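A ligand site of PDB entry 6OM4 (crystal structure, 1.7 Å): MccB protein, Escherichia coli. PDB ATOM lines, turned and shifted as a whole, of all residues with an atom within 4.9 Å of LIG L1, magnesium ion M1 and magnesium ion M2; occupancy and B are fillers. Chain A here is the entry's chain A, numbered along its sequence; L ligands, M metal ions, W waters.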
ATOM      1  N   GLY A 124      15.033 -26.175  -5.450  1.00  0.00           N
ATOM      2  CA  GLY A 124      15.516 -26.777  -6.659  1.00  0.00           C
ATOM      3  C   GLY A 124      14.454 -26.804  -7.747  1.00  0.00           C
ATOM      4  O   GLY A 124      13.709 -25.818  -7.933  1.00  0.00           O
ATOM      5  N   GLY A 125      14.336 -27.943  -8.447  1.00  0.00           N
ATOM      6  CA  GLY A 125      13.452 -27.987  -9.624  1.00  0.00           C
ATOM      7  C   GLY A 125      11.994 -27.706  -9.259  1.00  0.00           C
ATOM      8  O   GLY A 125      11.264 -26.873  -9.866  1.00  0.00           O
ATOM      9  N   ASP A 148      21.789 -24.681  -0.644  1.00  0.00           N
ATOM     10  CA  ASP A 148      22.621 -25.038  -1.778  1.00  0.00           C
ATOM     11  C   ASP A 148      22.998 -23.847  -2.668  1.00  0.00           C
ATOM     12  O   ASP A 148      22.341 -22.811  -2.720  1.00  0.00           O
ATOM     13  CB  ASP A 148      21.911 -26.087  -2.621  1.00  0.00           C
ATOM     14  CG  ASP A 148      22.799 -26.914  -3.538  1.00  0.00           C
ATOM     15  OD1 ASP A 148      24.044 -26.954  -3.310  1.00  0.00           O
ATOM     16  OD2 ASP A 148      22.234 -27.540  -4.468  1.00  0.00           O
ATOM     17  N   GLN A 149      24.047 -24.070  -3.446  1.00  0.00           N
ATOM     18  CA  GLN A 149      24.521 -23.154  -4.486  1.00  0.00           C
ATOM     19  C   GLN A 149      24.075 -23.669  -5.855  1.00  0.00           C
ATOM     20  O   GLN A 149      24.005 -24.906  -6.083  1.00  0.00           O
ATOM     21  CB  GLN A 149      26.040 -23.054  -4.458  1.00  0.00           C
ATOM     22  CG  GLN A 149      26.554 -22.330  -3.231  1.00  0.00           C
ATOM     23  CD  GLN A 149      26.268 -23.102  -1.969  1.00  0.00           C
ATOM     24  OE1 GLN A 149      26.537 -24.294  -1.878  1.00  0.00           O
ATOM     25  NE2 GLN A 149      25.696 -22.425  -0.977  1.00  0.00           N
ATOM     26  N   GLU A 151      24.368 -24.789  -9.626  1.00  0.00           N
ATOM     27  CA  GLU A 151      25.318 -25.470 -10.505  1.00  0.00           C
ATOM     28  C   GLU A 151      24.809 -25.462 -11.943  1.00  0.00           C
ATOM     29  O   GLU A 151      23.611 -25.379 -12.202  1.00  0.00           O
ATOM     30  CB  GLU A 151      25.547 -26.896 -10.027  1.00  0.00           C
ATOM     31  CG  GLU A 151      26.294 -26.942  -8.718  1.00  0.00           C
ATOM     32  CD  GLU A 151      26.407 -28.292  -8.063  1.00  0.00           C
ATOM     33  OE1 GLU A 151      25.942 -29.320  -8.635  1.00  0.00           O
ATOM     34  OE2 GLU A 151      26.928 -28.300  -6.943  1.00  0.00           O
ATOM     35  N   THR A 153      24.380 -27.807 -14.045  1.00  0.00           N
ATOM     36  CA  THR A 153      23.423 -28.903 -14.378  1.00  0.00           C
ATOM     37  C   THR A 153      21.990 -28.567 -13.924  1.00  0.00           C
ATOM     38  O   THR A 153      21.025 -29.114 -14.453  1.00  0.00           O
ATOM     39  CB  THR A 153      23.818 -30.256 -13.795  1.00  0.00           C
ATOM     40  OG1 THR A 153      23.763 -30.259 -12.368  1.00  0.00           O
ATOM     41  CG2 THR A 153      25.199 -30.675 -14.253  1.00  0.00           C
ATOM     42  N   ASN A 154      21.861 -27.630 -12.984  1.00  0.00           N
ATOM     43  CA  ASN A 154      20.568 -27.211 -12.472  1.00  0.00           C
ATOM     44  C   ASN A 154      19.712 -26.493 -13.525  1.00  0.00           C
ATOM     45  O   ASN A 154      18.472 -26.440 -13.396  1.00  0.00           O
ATOM     46  CB  ASN A 154      20.702 -26.281 -11.283  1.00  0.00           C
ATOM     47  CG  ASN A 154      21.223 -26.948 -10.030  1.00  0.00           C
ATOM     48  OD1 ASN A 154      21.182 -28.188  -9.876  1.00  0.00           O
ATOM     49  ND2 ASN A 154      21.719 -26.126  -9.149  1.00  0.00           N
ATOM     50  N   ARG A 157      16.054 -27.601 -15.364  1.00  0.00           N
ATOM     51  CA  ARG A 157      14.742 -27.596 -14.663  1.00  0.00           C
ATOM     52  C   ARG A 157      14.486 -26.310 -13.862  1.00  0.00           C
ATOM     53  O   ARG A 157      13.306 -25.927 -13.634  1.00  0.00           O
ATOM     54  CB  ARG A 157      14.664 -28.765 -13.662  1.00  0.00           C
ATOM     55  CG  ARG A 157      14.921 -30.156 -14.257  1.00  0.00           C
ATOM     56  CD  ARG A 157      15.463 -31.211 -13.297  1.00  0.00           C
ATOM     57  NE  ARG A 157      16.077 -30.681 -12.078  1.00  0.00           N
ATOM     58  CZ  ARG A 157      17.365 -30.718 -11.722  1.00  0.00           C
ATOM     59  NH1 ARG A 157      18.370 -30.475 -12.580  1.00  0.00           N
ATOM     60  NH2 ARG A 157      17.588 -31.034 -10.459  1.00  0.00           N
ATOM     61  N   GLN A 158      15.564 -25.643 -13.377  1.00  0.00           N
ATOM     62  CA  GLN A 158      15.472 -24.651 -12.314  1.00  0.00           C
ATOM     63  C   GLN A 158      15.405 -23.288 -13.003  1.00  0.00           C
ATOM     64  O   GLN A 158      16.394 -22.608 -13.159  1.00  0.00           O
ATOM     65  CB  GLN A 158      16.606 -24.822 -11.288  1.00  0.00           C
ATOM     66  CG  GLN A 158      16.510 -26.186 -10.628  1.00  0.00           C
ATOM     67  CD  GLN A 158      17.480 -26.599  -9.543  1.00  0.00           C
ATOM     68  OE1 GLN A 158      18.092 -25.777  -8.879  1.00  0.00           O
ATOM     69  NE2 GLN A 158      17.666 -27.894  -9.397  1.00  0.00           N
ATOM     70  N   LYS A 170      20.871 -20.431  -4.036  1.00  0.00           N
ATOM     71  CA  LYS A 170      19.537 -20.582  -4.641  1.00  0.00           C
ATOM     72  C   LYS A 170      18.518 -19.636  -4.026  1.00  0.00           C
ATOM     73  O   LYS A 170      17.714 -19.011  -4.777  1.00  0.00           O
ATOM     74  CB  LYS A 170      19.068 -22.037  -4.512  1.00  0.00           C
ATOM     75  CG  LYS A 170      19.922 -22.986  -5.323  1.00  0.00           C
ATOM     76  CD  LYS A 170      19.300 -24.345  -5.459  1.00  0.00           C
ATOM     77  CE  LYS A 170      20.211 -25.264  -6.229  1.00  0.00           C
ATOM     78  NZ  LYS A 170      19.568 -26.572  -6.448  1.00  0.00           N
ATOM     79  N   ASP A 214      14.437 -33.355  -0.546  1.00  0.00           N
ATOM     80  CA  ASP A 214      14.435 -34.785  -0.799  1.00  0.00           C
ATOM     81  C   ASP A 214      15.616 -35.561  -0.186  1.00  0.00           C
ATOM     82  O   ASP A 214      15.760 -36.735  -0.516  1.00  0.00           O
ATOM     83  CB  ASP A 214      14.439 -35.019  -2.304  1.00  0.00           C
ATOM     84  CG  ASP A 214      15.585 -34.338  -3.067  1.00  0.00           C
ATOM     85  OD1 ASP A 214      16.501 -33.776  -2.406  1.00  0.00           O
ATOM     86  OD2 ASP A 214      15.583 -34.422  -4.329  1.00  0.00           O
ATOM     87  N   LYS A 287      20.923 -40.963  -8.233  1.00  0.00           N
ATOM     88  CA  LYS A 287      20.601 -39.678  -8.823  1.00  0.00           C
ATOM     89  C   LYS A 287      19.385 -39.878  -9.726  1.00  0.00           C
ATOM     90  O   LYS A 287      19.394 -40.736 -10.606  1.00  0.00           O
ATOM     91  CB  LYS A 287      21.788 -39.129  -9.606  1.00  0.00           C
ATOM     92  CG  LYS A 287      23.048 -38.800  -8.798  1.00  0.00           C
ATOM     93  CD  LYS A 287      24.158 -38.184  -9.632  1.00  0.00           C
ATOM     94  CE  LYS A 287      24.447 -36.719  -9.384  1.00  0.00           C
ATOM     95  NZ  LYS A 287      23.443 -36.046  -8.521  1.00  0.00           N
HETATM   96  P1  LIG L   1      20.534 -32.240  -8.567  1.00  0.00           P
HETATM   97  O1  LIG L   1      20.165 -32.447 -10.035  1.00  0.00           O
HETATM   98  O2  LIG L   1      19.754 -33.129  -7.615  1.00  0.00           O
HETATM   99  O3  LIG L   1      22.025 -32.210  -8.252  1.00  0.00           O
HETATM  100  O4  LIG L   1      20.001 -30.742  -8.356  1.00  0.00           O
HETATM  101  P2  LIG L   1      19.896 -29.951  -6.938  1.00  0.00           P
HETATM  102  O5  LIG L   1      18.635 -29.143  -6.996  1.00  0.00           O
HETATM  103  O6  LIG L   1      19.896 -30.944  -5.819  1.00  0.00           O
HETATM  104  O7  LIG L   1      21.014 -29.008  -6.891  1.00  0.00           O
HETATM  105  O1  LG2 L   2      17.272 -31.826  -6.382  1.00  0.00           O
HETATM  106  P1  LG2 L   2      16.026 -31.031  -6.661  1.00  0.00           P
HETATM  107  O2  LG2 L   2      15.883 -30.376  -8.020  1.00  0.00           O
HETATM  108  N1  LG2 L   2      14.765 -32.152  -6.430  1.00  0.00           N
HETATM  109  O3  LG2 L   2      15.789 -29.865  -5.605  1.00  0.00           O
HETATM  110  C1  LG2 L   2      15.846 -30.249  -4.199  1.00  0.00           C
HETATM  111  C2  LG2 L   2      16.190 -28.952  -3.441  1.00  0.00           C
HETATM  112  C3  LG2 L   2      17.706 -28.614  -3.682  1.00  0.00           C
HETATM  113  O4  LG2 L   2      17.907 -27.314  -4.057  1.00  0.00           O
HETATM  114  C4  LG2 L   2      18.342 -29.100  -2.313  1.00  0.00           C
HETATM  115  O5  LG2 L   2      19.478 -28.216  -1.939  1.00  0.00           O
HETATM  116  C5  LG2 L   2      17.376 -28.944  -1.398  1.00  0.00           C
HETATM  117  O6  LG2 L   2      15.983 -29.193  -2.180  1.00  0.00           O
HETATM  118  N2  LG2 L   2      17.351 -29.873  -0.304  1.00  0.00           N
HETATM  119  C6  LG2 L   2      17.268 -29.548   1.015  1.00  0.00           C
HETATM  120  C7  LG2 L   2      17.238 -30.705   1.718  1.00  0.00           C
HETATM  121  N3  LG2 L   2      17.303 -31.731   0.842  1.00  0.00           N
HETATM  122  C8  LG2 L   2      17.347 -31.212  -0.372  1.00  0.00           C
HETATM  123  N4  LG2 L   2      17.214 -28.357   1.637  1.00  0.00           N
HETATM  124  C9  LG2 L   2      17.132 -28.321   2.933  1.00  0.00           C
HETATM  125  N5  LG2 L   2      17.120 -29.444   3.656  1.00  0.00           N
HETATM  126  C10 LG2 L   2      17.170 -30.623   3.091  1.00  0.00           C
HETATM  127  N6  LG2 L   2      17.162 -31.824   3.898  1.00  0.00           N
HETATM  128 MG    MG M   1      22.873 -28.837  -5.977  1.00  0.00          MG
HETATM  129 MG    MG M   2      18.982 -32.775  -5.820  1.00  0.00          MG
HETATM  130  O   HOH W   1      20.558 -35.773  -8.042  1.00  0.00           O
HETATM  131  O   HOH W   2      23.239 -27.153  -7.097  1.00  0.00           O
HETATM  132  O   HOH W   3      23.639 -30.131  -7.391  1.00  0.00           O
HETATM  133  O   HOH W   4      20.970 -30.488 -11.573  1.00  0.00           O
HETATM  134  O   HOH W   5      22.346 -30.547  -4.707  1.00  0.00           O
HETATM  135  O   HOH W   6      22.826 -33.911  -6.479  1.00  0.00           O
HETATM  136  O   HOH W   7      24.722 -28.673  -5.104  1.00  0.00           O
HETATM  137  O   HOH W   8      18.440 -32.504  -3.626  1.00  0.00           O
HETATM  138  O   HOH W   9      20.664 -33.806  -5.071  1.00  0.00           O
HETATM  139  O   HOH W  10      17.790 -34.565  -5.866  1.00  0.00           O
HETATM  140  O   HOH W  11      18.336 -34.102 -10.900  1.00  0.00           O
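Magnesium ion M1 is bound by water W7 (2.1 Å), water W2 (2.1 Å), water W3 (2.1 Å), O7 of LIG L1 (2.1 Å), OD2 of Asp 148 (2.1 Å) and water W5 (2.2 Å).
No residue comes within 4 Å of magnesium ion M2.
Magnesium ion M2 is bound by O2 of LIG L1 (2.0 Å), O1 of LG2 L2 (2.0 Å), O6 of LIG L1 (2.0 Å), water W9 (2.1 Å), water W10 (2.2 Å) and water W8 (2.3 Å). Magnesium ion M2 has six donor atoms within binding distance.
NZ of Lys 170 is in salt-bridge range of O5 of LIG L1, 2.8 Å away. The side-chain amide nitrogen (NE2) of Gln 158 is in hydrogen-bond range of an oxygen (O5) of LIG L1 (2.9 Å). NH2 of Arg 157 is in salt-bridge range of O1 of LIG L1. An oxygen (O4) of LIG L1 lies close to the side-chain amide oxygen of Asn 154 (3.2 Å). O4 of LG2 L2 sits at hydrogen-bond distance from NZ of Lys 170 (3.0 Å). NE2 of Gln 158 is in hydrogen-bond range of O2 of LG2 L2. NH2 of Arg 157 lies within salt-bridge range of O2 of LG2 L2. The backbone NH (N) of Gly 124 sits at hydrogen-bond distance from an oxygen (O4) of LG2 L2 (3.4 Å). The side-chain carboxylate (OD2) of Asp 214 lies within hydrogen-bond range of a nitrogen (N1) of LG2 L2, 3.2 Å away. The backbone NH of Gly 125 sits at hydrogen-bond distance from an oxygen (O2) of LG2 L2, 2.9 Å away.
O of Asp 148 sits at hydrogen-bond distance from N of Lys 170. NZ of Lys 170 is in hydrogen-bond range of OE1 of Gln 158, 3.0 Å away. The side-chain amino group (NZ) of Lys 170 sits close to the side-chain amide nitrogen (ND2) of Asn 154 (3.5 Å). The guanidinium group of Arg 157 lies close to the side-chain amide nitrogen of Gln 158, at 3.3 Å. The side-chain amide nitrogen (NE2) of Gln 158 lies close to the backbone NH (N) of Gly 125. The backbone NH (N) of Glu 151 sits close to the side-chain amide nitrogen (ND2) of Asn 154 (3.0 Å).
Water W3 bridges OE1 of Glu 151 (2.7 Å) and O3 of LIG L1 (2.8 Å). Water W7 lies within hydrogen-bond range of OD1 of Asp 148 (2.6 Å) and OE2 of Glu 151 (2.9 Å). Water W2 bridges O of Gln 149 (2.6 Å) and ND2 of Asn 154 (2.8 Å). Water W6 lies within hydrogen-bond range of an oxygen (O3) of LIG L1 (2.6 Å) and the side-chain amino group of Lys 287 (3.0 Å). Water W11 lies within hydrogen-bond range of an oxygen (O1) of LIG L1 (2.6 Å) and the guanidinium group (NH2) of Arg 157 (3.2 Å). Water W4 lies within hydrogen-bond range of an oxygen (O1) of LIG L1 (2.6 Å), the guanidinium group (NH1) of Arg 157 (2.8 Å), the side-chain amide oxygen (OD1) of Asn 154 (2.9 Å) and the side-chain hydroxyl (OG1) of Thr 153 (2.9 Å).
Within 4 Å of magnesium ion M1: Asp 148. The nearest printed residue that does not touch magnesium ion M1 is Lys 170 (4.03 Å).
Residues that only touch LIG L1: Gly 124. Within 4 Å of LIG L1: Gly 124, Asp 148, Asn 154, Arg 157, Gln 158 and Lys 170.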
